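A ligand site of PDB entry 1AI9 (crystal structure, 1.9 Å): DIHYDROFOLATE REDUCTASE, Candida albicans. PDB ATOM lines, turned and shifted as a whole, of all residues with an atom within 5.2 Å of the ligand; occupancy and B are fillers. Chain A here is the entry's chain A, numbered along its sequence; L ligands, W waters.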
ATOM      1  N   VAL A  10      25.411  -1.114 -29.446  1.00  0.00           N
ATOM      2  CA  VAL A  10      26.679  -1.525 -28.860  1.00  0.00           C
ATOM      3  C   VAL A  10      27.444  -2.518 -29.751  1.00  0.00           C
ATOM      4  O   VAL A  10      26.793  -3.225 -30.530  1.00  0.00           O
ATOM      5  CB  VAL A  10      26.445  -2.186 -27.469  1.00  0.00           C
ATOM      6  CG1 VAL A  10      25.666  -3.535 -27.552  1.00  0.00           C
ATOM      7  CG2 VAL A  10      27.719  -2.418 -26.662  1.00  0.00           C
ATOM      8  N   ALA A  11      28.760  -2.586 -29.648  1.00  0.00           N
ATOM      9  CA  ALA A  11      29.688  -3.485 -30.242  1.00  0.00           C
ATOM     10  C   ALA A  11      30.338  -4.341 -29.091  1.00  0.00           C
ATOM     11  O   ALA A  11      30.896  -3.737 -28.205  1.00  0.00           O
ATOM     12  CB  ALA A  11      30.870  -2.761 -30.939  1.00  0.00           C
ATOM     13  N   ALA A  12      30.257  -5.631 -29.204  1.00  0.00           N
ATOM     14  CA  ALA A  12      30.776  -6.529 -28.110  1.00  0.00           C
ATOM     15  C   ALA A  12      31.531  -7.716 -28.734  1.00  0.00           C
ATOM     16  O   ALA A  12      31.117  -8.233 -29.790  1.00  0.00           O
ATOM     17  CB  ALA A  12      29.513  -7.035 -27.398  1.00  0.00           C
ATOM     18  N   ILE A  19      33.349  -5.240 -23.733  1.00  0.00           N
ATOM     19  CA  ILE A  19      33.162  -3.904 -24.323  1.00  0.00           C
ATOM     20  C   ILE A  19      34.234  -2.862 -24.198  1.00  0.00           C
ATOM     21  O   ILE A  19      34.120  -1.739 -24.787  1.00  0.00           O
ATOM     22  CB  ILE A  19      31.792  -3.392 -23.724  1.00  0.00           C
ATOM     23  CG1 ILE A  19      30.682  -3.572 -24.720  1.00  0.00           C
ATOM     24  CG2 ILE A  19      31.634  -2.365 -22.655  1.00  0.00           C
ATOM     25  CD1 ILE A  19      30.281  -5.017 -24.860  1.00  0.00           C
ATOM     26  N   GLY A  20      35.183  -3.100 -23.322  1.00  0.00           N
ATOM     27  CA  GLY A  20      36.244  -2.157 -23.053  1.00  0.00           C
ATOM     28  C   GLY A  20      37.266  -2.614 -22.035  1.00  0.00           C
ATOM     29  O   GLY A  20      37.240  -3.701 -21.453  1.00  0.00           O
ATOM     30  N   TYR A  21      38.219  -1.691 -21.890  1.00  0.00           N
ATOM     31  CA  TYR A  21      39.374  -1.873 -20.972  1.00  0.00           C
ATOM     32  C   TYR A  21      39.892  -0.482 -20.621  1.00  0.00           C
ATOM     33  O   TYR A  21      40.158   0.306 -21.556  1.00  0.00           O
ATOM     34  CB  TYR A  21      40.404  -2.693 -21.763  1.00  0.00           C
ATOM     35  CG  TYR A  21      41.647  -3.046 -21.001  1.00  0.00           C
ATOM     36  CD1 TYR A  21      41.701  -4.162 -20.176  1.00  0.00           C
ATOM     37  CD2 TYR A  21      42.802  -2.261 -21.131  1.00  0.00           C
ATOM     38  CE1 TYR A  21      42.857  -4.516 -19.488  1.00  0.00           C
ATOM     39  CE2 TYR A  21      43.980  -2.593 -20.463  1.00  0.00           C
ATOM     40  CZ  TYR A  21      43.998  -3.711 -19.632  1.00  0.00           C
ATOM     41  OH  TYR A  21      45.133  -4.051 -18.946  1.00  0.00           O
ATOM     42  N   LYS A  22      40.014  -0.180 -19.341  1.00  0.00           N
ATOM     43  CA  LYS A  22      40.447   1.148 -18.847  1.00  0.00           C
ATOM     44  C   LYS A  22      39.247   2.091 -18.877  1.00  0.00           C
ATOM     45  O   LYS A  22      38.760   2.588 -17.829  1.00  0.00           O
ATOM     46  CB  LYS A  22      41.656   1.729 -19.552  1.00  0.00           C
ATOM     47  CG  LYS A  22      41.856   3.213 -19.748  1.00  0.00           C
ATOM     48  CD  LYS A  22      42.667   3.977 -18.740  1.00  0.00           C
ATOM     49  CE  LYS A  22      44.137   3.995 -19.148  1.00  0.00           C
ATOM     50  NZ  LYS A  22      44.938   4.820 -18.200  1.00  0.00           N
ATOM     51  N   GLY A  23      38.831   2.353 -20.091  1.00  0.00           N
ATOM     52  CA  GLY A  23      37.738   3.261 -20.439  1.00  0.00           C
ATOM     53  C   GLY A  23      37.796   3.448 -21.973  1.00  0.00           C
ATOM     54  O   GLY A  23      37.330   4.489 -22.444  1.00  0.00           O
ATOM     55  N   LYS A  24      38.331   2.448 -22.645  1.00  0.00           N
ATOM     56  CA  LYS A  24      38.482   2.428 -24.101  1.00  0.00           C
ATOM     57  C   LYS A  24      38.051   1.107 -24.735  1.00  0.00           C
ATOM     58  O   LYS A  24      38.151   0.037 -24.112  1.00  0.00           O
ATOM     59  CB  LYS A  24      39.884   2.785 -24.503  1.00  0.00           C
ATOM     60  CG  LYS A  24      41.118   2.047 -24.077  1.00  0.00           C
ATOM     61  CD  LYS A  24      41.259   0.627 -24.550  1.00  0.00           C
ATOM     62  CE  LYS A  24      42.366  -0.228 -24.062  1.00  0.00           C
ATOM     63  NZ  LYS A  24      43.553  -0.194 -24.963  1.00  0.00           N
ATOM     64  N   MET A  25      37.690   1.158 -26.001  1.00  0.00           N
ATOM     65  CA  MET A  25      37.327  -0.097 -26.741  1.00  0.00           C
ATOM     66  C   MET A  25      38.668  -0.711 -27.181  1.00  0.00           C
ATOM     67  O   MET A  25      39.522  -0.005 -27.735  1.00  0.00           O
ATOM     68  CB  MET A  25      36.448   0.221 -27.957  1.00  0.00           C
ATOM     69  CG  MET A  25      35.207   0.956 -27.591  1.00  0.00           C
ATOM     70  SD  MET A  25      34.465   1.750 -29.064  1.00  0.00           S
ATOM     71  CE  MET A  25      33.705   0.327 -29.862  1.00  0.00           C
ATOM     72  N   TRP A  27      39.671  -2.226 -29.711  1.00  0.00           N
ATOM     73  CA  TRP A  27      39.756  -2.348 -31.162  1.00  0.00           C
ATOM     74  C   TRP A  27      39.429  -1.033 -31.857  1.00  0.00           C
ATOM     75  O   TRP A  27      38.805  -0.141 -31.270  1.00  0.00           O
ATOM     76  CB  TRP A  27      38.708  -3.418 -31.682  1.00  0.00           C
ATOM     77  CG  TRP A  27      37.328  -3.198 -31.128  1.00  0.00           C
ATOM     78  CD1 TRP A  27      36.402  -2.252 -31.447  1.00  0.00           C
ATOM     79  CD2 TRP A  27      36.771  -3.962 -30.026  1.00  0.00           C
ATOM     80  NE1 TRP A  27      35.290  -2.393 -30.626  1.00  0.00           N
ATOM     81  CE2 TRP A  27      35.515  -3.403 -29.746  1.00  0.00           C
ATOM     82  CE3 TRP A  27      37.211  -5.062 -29.304  1.00  0.00           C
ATOM     83  CZ2 TRP A  27      34.671  -3.930 -28.752  1.00  0.00           C
ATOM     84  CZ3 TRP A  27      36.381  -5.561 -28.313  1.00  0.00           C
ATOM     85  CH2 TRP A  27      35.152  -5.009 -28.042  1.00  0.00           C
ATOM     86  N   MET A  54      23.684   9.042 -23.425  1.00  0.00           N
ATOM     87  CA  MET A  54      24.922   8.544 -22.835  1.00  0.00           C
ATOM     88  C   MET A  54      25.098   8.866 -21.387  1.00  0.00           C
ATOM     89  O   MET A  54      24.525   9.911 -20.861  1.00  0.00           O
ATOM     90  CB  MET A  54      26.159   8.934 -23.739  1.00  0.00           C
ATOM     91  CG  MET A  54      26.395  10.472 -23.476  1.00  0.00           C
ATOM     92  SD  MET A  54      27.616  10.893 -24.824  1.00  0.00           S
ATOM     93  CE  MET A  54      26.415  11.458 -26.007  1.00  0.00           C
ATOM     94  N   GLY A  55      25.898   8.149 -20.661  1.00  0.00           N
ATOM     95  CA  GLY A  55      26.296   8.373 -19.273  1.00  0.00           C
ATOM     96  C   GLY A  55      27.354   9.535 -19.309  1.00  0.00           C
ATOM     97  O   GLY A  55      28.010   9.789 -20.322  1.00  0.00           O
ATOM     98  N   ARG A  56      27.419  10.156 -18.139  1.00  0.00           N
ATOM     99  CA  ARG A  56      28.368  11.299 -17.955  1.00  0.00           C
ATOM    100  C   ARG A  56      29.782  10.879 -18.311  1.00  0.00           C
ATOM    101  O   ARG A  56      30.468  11.678 -18.963  1.00  0.00           O
ATOM    102  CB  ARG A  56      28.315  11.783 -16.494  1.00  0.00           C
ATOM    103  CG  ARG A  56      29.251  13.006 -16.250  1.00  0.00           C
ATOM    104  CD  ARG A  56      29.341  13.328 -14.785  1.00  0.00           C
ATOM    105  NE  ARG A  56      29.814  12.306 -13.936  1.00  0.00           N
ATOM    106  CZ  ARG A  56      30.846  11.534 -13.764  1.00  0.00           C
ATOM    107  NH1 ARG A  56      31.951  11.567 -14.564  1.00  0.00           N
ATOM    108  NH2 ARG A  56      30.940  10.675 -12.754  1.00  0.00           N
ATOM    109  N   LYS A  57      30.288   9.761 -17.910  1.00  0.00           N
ATOM    110  CA  LYS A  57      31.643   9.317 -18.239  1.00  0.00           C
ATOM    111  C   LYS A  57      31.916   9.175 -19.758  1.00  0.00           C
ATOM    112  O   LYS A  57      32.993   9.591 -20.170  1.00  0.00           O
ATOM    113  CB  LYS A  57      32.070   8.025 -17.587  1.00  0.00           C
ATOM    114  CG  LYS A  57      32.159   8.057 -16.070  1.00  0.00           C
ATOM    115  CD  LYS A  57      32.318   6.598 -15.578  1.00  0.00           C
ATOM    116  CE  LYS A  57      32.501   6.500 -14.090  1.00  0.00           C
ATOM    117  NZ  LYS A  57      31.469   7.213 -13.310  1.00  0.00           N
ATOM    118  N   THR A  58      31.013   8.603 -20.481  1.00  0.00           N
ATOM    119  CA  THR A  58      31.130   8.459 -21.956  1.00  0.00           C
ATOM    120  C   THR A  58      31.250   9.877 -22.524  1.00  0.00           C
ATOM    121  O   THR A  58      32.187  10.122 -23.359  1.00  0.00           O
ATOM    122  CB  THR A  58      30.076   7.569 -22.643  1.00  0.00           C
ATOM    123  OG1 THR A  58      30.144   6.206 -22.087  1.00  0.00           O
ATOM    124  CG2 THR A  58      30.266   7.470 -24.215  1.00  0.00           C
ATOM    125  N   LEU A  77      23.248  11.600 -19.069  1.00  0.00           N
ATOM    126  CA  LEU A  77      22.724  11.277 -17.764  1.00  0.00           C
ATOM    127  C   LEU A  77      23.768  11.234 -16.667  1.00  0.00           C
ATOM    128  O   LEU A  77      24.830  10.567 -16.724  1.00  0.00           O
ATOM    129  CB  LEU A  77      21.959   9.909 -17.788  1.00  0.00           C
ATOM    130  CG  LEU A  77      20.900   9.709 -18.823  1.00  0.00           C
ATOM    131  CD1 LEU A  77      20.416   8.194 -18.759  1.00  0.00           C
ATOM    132  CD2 LEU A  77      19.651  10.541 -18.792  1.00  0.00           C
ATOM    133  N   SER A  78      23.304  11.750 -15.523  1.00  0.00           N
ATOM    134  CA  SER A  78      24.093  11.656 -14.274  1.00  0.00           C
ATOM    135  C   SER A  78      23.093  11.774 -13.118  1.00  0.00           C
ATOM    136  O   SER A  78      22.181  12.579 -13.234  1.00  0.00           O
ATOM    137  CB  SER A  78      25.075  12.779 -14.228  1.00  0.00           C
ATOM    138  OG  SER A  78      25.517  13.160 -12.976  1.00  0.00           O
ATOM    139  N   ARG A  79      23.373  11.055 -12.080  1.00  0.00           N
ATOM    140  CA  ARG A  79      22.500  11.148 -10.846  1.00  0.00           C
ATOM    141  C   ARG A  79      22.574  12.485 -10.164  1.00  0.00           C
ATOM    142  O   ARG A  79      21.610  12.907  -9.450  1.00  0.00           O
ATOM    143  CB  ARG A  79      22.709   9.860 -10.088  1.00  0.00           C
ATOM    144  CG  ARG A  79      22.092   8.591 -10.698  1.00  0.00           C
ATOM    145  CD  ARG A  79      22.361   7.381  -9.916  1.00  0.00           C
ATOM    146  NE  ARG A  79      23.400   6.471 -10.259  1.00  0.00           N
ATOM    147  CZ  ARG A  79      24.701   6.703 -10.356  1.00  0.00           C
ATOM    148  NH1 ARG A  79      25.210   7.904 -10.060  1.00  0.00           N
ATOM    149  NH2 ARG A  79      25.544   5.815 -10.843  1.00  0.00           N
ATOM    150  N   SER A  80      23.558  13.329 -10.439  1.00  0.00           N
ATOM    151  CA  SER A  80      23.696  14.686  -9.884  1.00  0.00           C
ATOM    152  C   SER A  80      23.065  15.790 -10.695  1.00  0.00           C
ATOM    153  O   SER A  80      23.129  17.046 -10.394  1.00  0.00           O
ATOM    154  CB  SER A  80      25.238  15.019  -9.891  1.00  0.00           C
ATOM    155  OG  SER A  80      25.814  14.079  -9.011  1.00  0.00           O
ATOM    156  N   SER A  94      18.735  13.251 -15.124  1.00  0.00           N
ATOM    157  CA  SER A  94      19.080  12.204 -14.177  1.00  0.00           C
ATOM    158  C   SER A  94      18.369  10.875 -14.465  1.00  0.00           C
ATOM    159  O   SER A  94      18.685   9.909 -13.720  1.00  0.00           O
ATOM    160  CB  SER A  94      18.738  12.626 -12.726  1.00  0.00           C
ATOM    161  OG  SER A  94      17.420  13.190 -12.730  1.00  0.00           O
ATOM    162  N   SER A  95      17.424  10.849 -15.343  1.00  0.00           N
ATOM    163  CA  SER A  95      16.698   9.654 -15.741  1.00  0.00           C
ATOM    164  C   SER A  95      16.362   9.732 -17.259  1.00  0.00           C
ATOM    165  O   SER A  95      16.062  10.810 -17.747  1.00  0.00           O
ATOM    166  CB  SER A  95      15.499   9.344 -14.949  1.00  0.00           C
ATOM    167  OG  SER A  95      14.352  10.085 -15.164  1.00  0.00           O
ATOM    168  N   ILE A 112      23.691   4.935 -26.322  1.00  0.00           N
ATOM    169  CA  ILE A 112      25.013   4.699 -26.897  1.00  0.00           C
ATOM    170  C   ILE A 112      26.101   4.424 -25.898  1.00  0.00           C
ATOM    171  O   ILE A 112      27.304   4.376 -26.269  1.00  0.00           O
ATOM    172  CB  ILE A 112      25.371   5.850 -27.945  1.00  0.00           C
ATOM    173  CG1 ILE A 112      25.700   7.165 -27.242  1.00  0.00           C
ATOM    174  CG2 ILE A 112      24.188   5.891 -28.991  1.00  0.00           C
ATOM    175  CD1 ILE A 112      26.693   8.169 -27.923  1.00  0.00           C
ATOM    176  N   GLY A 113      25.727   4.193 -24.613  1.00  0.00           N
ATOM    177  CA  GLY A 113      26.771   3.807 -23.631  1.00  0.00           C
ATOM    178  C   GLY A 113      26.777   4.771 -22.430  1.00  0.00           C
ATOM    179  O   GLY A 113      25.984   5.703 -22.406  1.00  0.00           O
ATOM    180  N   GLY A 114      27.612   4.479 -21.485  1.00  0.00           N
ATOM    181  CA  GLY A 114      28.618   3.426 -21.369  1.00  0.00           C
ATOM    182  C   GLY A 114      28.107   2.106 -20.785  1.00  0.00           C
ATOM    183  O   GLY A 114      26.905   1.795 -20.766  1.00  0.00           O
ATOM    184  N   ALA A 115      29.061   1.384 -20.217  1.00  0.00           N
ATOM    185  CA  ALA A 115      28.777   0.039 -19.645  1.00  0.00           C
ATOM    186  C   ALA A 115      27.738   0.092 -18.532  1.00  0.00           C
ATOM    187  O   ALA A 115      26.826  -0.781 -18.571  1.00  0.00           O
ATOM    188  CB  ALA A 115      30.067  -0.522 -19.056  1.00  0.00           C
ATOM    189  N   GLU A 116      27.886   1.009 -17.584  1.00  0.00           N
ATOM    190  CA  GLU A 116      26.879   1.066 -16.515  1.00  0.00           C
ATOM    191  C   GLU A 116      25.525   1.380 -17.052  1.00  0.00           C
ATOM    192  O   GLU A 116      24.438   0.862 -16.634  1.00  0.00           O
ATOM    193  CB  GLU A 116      27.323   2.002 -15.390  1.00  0.00           C
ATOM    194  CG  GLU A 116      26.359   2.214 -14.249  1.00  0.00           C
ATOM    195  CD  GLU A 116      26.783   3.002 -13.060  1.00  0.00           C
ATOM    196  OE1 GLU A 116      27.938   3.523 -13.114  1.00  0.00           O
ATOM    197  OE2 GLU A 116      26.024   3.094 -12.084  1.00  0.00           O
ATOM    198  N   ILE A 117      25.487   2.369 -17.953  1.00  0.00           N
ATOM    199  CA  ILE A 117      24.191   2.750 -18.600  1.00  0.00           C
ATOM    200  C   ILE A 117      23.584   1.532 -19.338  1.00  0.00           C
ATOM    201  O   ILE A 117      22.356   1.278 -19.234  1.00  0.00           O
ATOM    202  CB  ILE A 117      24.489   3.976 -19.516  1.00  0.00           C
ATOM    203  CG1 ILE A 117      24.819   5.222 -18.709  1.00  0.00           C
ATOM    204  CG2 ILE A 117      23.500   4.219 -20.654  1.00  0.00           C
ATOM    205  CD1 ILE A 117      23.560   5.820 -17.891  1.00  0.00           C
ATOM    206  N   TYR A 118      24.408   0.805 -20.037  1.00  0.00           N
ATOM    207  CA  TYR A 118      23.988  -0.367 -20.785  1.00  0.00           C
ATOM    208  C   TYR A 118      23.350  -1.459 -19.840  1.00  0.00           C
ATOM    209  O   TYR A 118      22.193  -1.804 -20.054  1.00  0.00           O
ATOM    210  CB  TYR A 118      24.986  -1.091 -21.635  1.00  0.00           C
ATOM    211  CG  TYR A 118      25.525  -0.403 -22.848  1.00  0.00           C
ATOM    212  CD1 TYR A 118      24.653   0.148 -23.839  1.00  0.00           C
ATOM    213  CD2 TYR A 118      26.885  -0.410 -23.102  1.00  0.00           C
ATOM    214  CE1 TYR A 118      25.169   0.673 -25.007  1.00  0.00           C
ATOM    215  CE2 TYR A 118      27.422   0.128 -24.288  1.00  0.00           C
ATOM    216  CZ  TYR A 118      26.557   0.594 -25.236  1.00  0.00           C
ATOM    217  OH  TYR A 118      26.997   1.193 -26.419  1.00  0.00           O
ATOM    218  N   GLU A 120      22.297  -1.211 -16.795  1.00  0.00           N
ATOM    219  CA  GLU A 120      21.116  -0.711 -16.104  1.00  0.00           C
ATOM    220  C   GLU A 120      19.879  -0.619 -16.984  1.00  0.00           C
ATOM    221  O   GLU A 120      18.789  -1.131 -16.627  1.00  0.00           O
ATOM    222  CB  GLU A 120      21.410   0.753 -15.628  1.00  0.00           C
ATOM    223  CG  GLU A 120      20.646   1.248 -14.420  1.00  0.00           C
ATOM    224  CD  GLU A 120      21.136   0.589 -13.143  1.00  0.00           C
ATOM    225  OE1 GLU A 120      22.203   0.868 -12.592  1.00  0.00           O
ATOM    226  OE2 GLU A 120      20.307  -0.279 -12.800  1.00  0.00           O
ATOM    227  N   LEU A 121      20.044   0.017 -18.145  1.00  0.00           N
ATOM    228  CA  LEU A 121      18.916   0.277 -19.066  1.00  0.00           C
ATOM    229  C   LEU A 121      18.346  -0.868 -19.777  1.00  0.00           C
ATOM    230  O   LEU A 121      17.230  -0.903 -20.397  1.00  0.00           O
ATOM    231  CB  LEU A 121      19.176   1.616 -19.681  1.00  0.00           C
ATOM    232  CG  LEU A 121      18.885   2.898 -19.035  1.00  0.00           C
ATOM    233  CD1 LEU A 121      19.113   3.136 -17.592  1.00  0.00           C
ATOM    234  CD2 LEU A 121      19.574   4.026 -19.875  1.00  0.00           C
ATOM    235  N   THR A 147      35.607  -4.885 -18.843  1.00  0.00           N
ATOM    236  CA  THR A 147      34.188  -4.497 -18.916  1.00  0.00           C
ATOM    237  C   THR A 147      33.342  -5.344 -19.820  1.00  0.00           C
ATOM    238  O   THR A 147      33.702  -5.648 -20.991  1.00  0.00           O
ATOM    239  CB  THR A 147      34.077  -2.979 -19.429  1.00  0.00           C
ATOM    240  OG1 THR A 147      35.294  -2.338 -18.907  1.00  0.00           O
ATOM    241  CG2 THR A 147      32.865  -2.351 -18.750  1.00  0.00           C
HETATM  242  P1  LIG L   1      29.141   5.383 -18.499  1.00  0.00           P
HETATM  243  O1  LIG L   1      29.098   6.122 -19.745  1.00  0.00           O
HETATM  244  O2  LIG L   1      28.125   4.297 -18.422  1.00  0.00           O
HETATM  245  O3  LIG L   1      28.836   6.334 -17.254  1.00  0.00           O
HETATM  246  C1  LIG L   1      28.369   5.929 -15.941  1.00  0.00           C
HETATM  247  C2  LIG L   1      27.848   7.249 -15.322  1.00  0.00           C
HETATM  248  O4  LIG L   1      26.550   7.524 -15.889  1.00  0.00           O
HETATM  249  C3  LIG L   1      27.614   7.138 -13.781  1.00  0.00           C
HETATM  250  O5  LIG L   1      28.896   7.256 -13.123  1.00  0.00           O
HETATM  251  C4  LIG L   1      26.541   8.226 -13.594  1.00  0.00           C
HETATM  252  O6  LIG L   1      26.907   9.607 -13.529  1.00  0.00           O
HETATM  253  C5  LIG L   1      25.741   8.046 -14.860  1.00  0.00           C
HETATM  254  N1  LIG L   1      24.724   7.081 -14.629  1.00  0.00           N
HETATM  255  C6  LIG L   1      24.931   5.724 -14.540  1.00  0.00           C
HETATM  256  N2  LIG L   1      23.807   5.058 -14.366  1.00  0.00           N
HETATM  257  C7  LIG L   1      22.858   6.053 -14.378  1.00  0.00           C
HETATM  258  C8  LIG L   1      21.451   5.982 -14.223  1.00  0.00           C
HETATM  259  N3  LIG L   1      20.922   4.776 -14.043  1.00  0.00           N
HETATM  260  N4  LIG L   1      20.752   7.119 -14.271  1.00  0.00           N
HETATM  261  C9  LIG L   1      21.456   8.309 -14.423  1.00  0.00           C
HETATM  262  N5  LIG L   1      22.729   8.467 -14.542  1.00  0.00           N
HETATM  263  C10 LIG L   1      23.407   7.312 -14.499  1.00  0.00           C
HETATM  264  O7  LIG L   1      30.519   4.829 -18.113  1.00  0.00           O
HETATM  265  P2  LIG L   1      31.290   3.474 -17.832  1.00  0.00           P
HETATM  266  O8  LIG L   1      32.620   3.774 -17.201  1.00  0.00           O
HETATM  267  O9  LIG L   1      30.490   2.579 -16.937  1.00  0.00           O
HETATM  268  O10 LIG L   1      31.449   2.782 -19.243  1.00  0.00           O
HETATM  269  C11 LIG L   1      32.618   3.151 -20.034  1.00  0.00           C
HETATM  270  C12 LIG L   1      33.111   1.875 -20.750  1.00  0.00           C
HETATM  271  O11 LIG L   1      32.118   1.571 -21.776  1.00  0.00           O
HETATM  272  C13 LIG L   1      34.435   2.129 -21.419  1.00  0.00           C
HETATM  273  O12 LIG L   1      35.469   1.169 -21.414  1.00  0.00           O
HETATM  274  C14 LIG L   1      33.949   2.376 -22.879  1.00  0.00           C
HETATM  275  O13 LIG L   1      35.056   2.081 -23.730  1.00  0.00           O
HETATM  276  C15 LIG L   1      32.787   1.407 -22.990  1.00  0.00           C
HETATM  277  N6  LIG L   1      31.856   1.670 -24.131  1.00  0.00           N
HETATM  278  C16 LIG L   1      31.812   0.702 -25.118  1.00  0.00           C
HETATM  279  C17 LIG L   1      31.007   0.859 -26.211  1.00  0.00           C
HETATM  280  C18 LIG L   1      31.030  -0.303 -27.298  1.00  0.00           C
HETATM  281  O14 LIG L   1      30.281  -0.280 -28.251  1.00  0.00           O
HETATM  282  N7  LIG L   1      31.949  -1.290 -27.107  1.00  0.00           N
HETATM  283  C19 LIG L   1      30.175   1.992 -26.376  1.00  0.00           C
HETATM  284  C20 LIG L   1      30.238   2.889 -25.277  1.00  0.00           C
HETATM  285  C21 LIG L   1      31.052   2.808 -24.169  1.00  0.00           C
HETATM  286  P3  LIG L   1      27.065  10.242 -12.021  1.00  0.00           P
HETATM  287  O15 LIG L   1      27.426  11.710 -12.413  1.00  0.00           O
HETATM  288  O16 LIG L   1      25.818  10.016 -11.348  1.00  0.00           O
HETATM  289  O17 LIG L   1      28.236   9.561 -11.458  1.00  0.00           O
HETATM  290  O   HOH W   1      20.974   3.847 -10.713  1.00  0.00           O
HETATM  291  O   HOH W   2      30.425   3.716 -13.984  1.00  0.00           O
HETATM  292  O   HOH W   3      35.363   3.311 -16.835  1.00  0.00           O
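Merely in contact with the ligand: Gly 23 (3.2 Å), Leu 77 (3.3 Å), Ser 94 (3.3 Å), Tyr 118 (3.3 Å), Ile 112 (3.4 Å), Gly 55 (3.5 Å), Glu 120 (3.6 Å), Met 25 (3.6 Å), Val 10 (3.7 Å), Gly 20 (3.8 Å), Gly 113 (3.8 Å) and Tyr 21 (3.996 Å).
Hydrophobic or aromatic side chains within 4 Å of the ligand: Val 10, Ala 11, Ile 19, Met 25, Leu 77, Ala 115, Ile 117 and Tyr 118.
Within 4 Å of the ligand: Val 10, Ala 11, Ile 19, Gly 20, Tyr 21, Gly 23, Lys 24, Met 25, Gly 55, Arg 56, Lys 57, Thr 58, Leu 77, Ser 78, Arg 79, Ser 94, Ile 112, Gly 113, Gly 114, Ala 115, Glu 116, Ile 117, Tyr 118 and Glu 120.
The nearest printed residue that does not touch the ligand is Ser 80 (4.1 Å).
Water W2 bridges the side-chain carboxylate of Glu 116 (2.6 Å) and an oxygen (O9) of the ligand (3.2 Å).
An oxygen (O5) of the ligand sits at hydrogen-bond distance from the side-chain amino group of Lys 57, 2.6 Å away.
O10 of the ligand is in hydrogen-bond range of N of Ala 115 (2.9 Å).
N5 of the ligand lies within hydrogen-bond range of N of Ser 78 (3.5 Å).
The backbone NH of Arg 79 lies within hydrogen-bond range of an oxygen (O16) of the ligand (2.8 Å).
The backbone NH (N) of Gly 114 is in hydrogen-bond range of an oxygen (O1) of the ligand (2.8 Å).
OG of Ser 78 is in hydrogen-bond range of O15 of the ligand, at 2.5 Å.
NE of Arg 56 is in salt-bridge range of O15 of the ligand (2.9 Å).
O1 of the ligand lies within hydrogen-bond range of OG1 of Thr 58.
The backbone NH of Lys 24 lies within hydrogen-bond range of an oxygen (O12) of the ligand (3.4 Å).
O of Ile 19 is in hydrogen-bond range of N7 of the ligand.
O14 of the ligand lies within hydrogen-bond range of N of Ala 11, 3.1 Å away.
NH1 of Arg 79 is in salt-bridge range of O16 of the ligand (2.5 Å).
O of Ala 11 sits at hydrogen-bond distance from N7 of the ligand (2.9 Å).
N of Ile 117 is in hydrogen-bond range of O2 of the ligand (3.3 Å).
N of Thr 58 lies within hydrogen-bond range of O1 of the ligand (3.2 Å).
The backbone NH (N) of Glu 116 lies within hydrogen-bond range of an oxygen (O9) of the ligand.
The backbone carbonyl oxygen of Ile 112 is in hydrogen-bond range of the side-chain hydroxyl of Tyr 118.
The guanidinium group (NH2) of Arg 79 is in salt-bridge range of the side-chain carboxylate (OE2) of Glu 116, 3.0 Å away.
The backbone NH (N) of Gly 55 lies within hydrogen-bond range of the backbone carbonyl oxygen (O) of Gly 113, at 3.0 Å.
O of Gly 20 sits at hydrogen-bond distance from N of Thr 147, 3.3 Å away.
N of Arg 56 sits at hydrogen-bond distance from O of Leu 77, 3.0 Å away.
The side-chain hydroxyl of Ser 78 sits close to the backbone NH of Ser 80 (3.2 Å).
The backbone NH (N) of Ile 19 is in hydrogen-bond range of the backbone carbonyl oxygen (O) of Thr 147, at 2.8 Å.
The side-chain hydroxyl (OG1) of Thr 58 lies within hydrogen-bond range of the backbone NH (N) of Gly 114 (3.1 Å).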
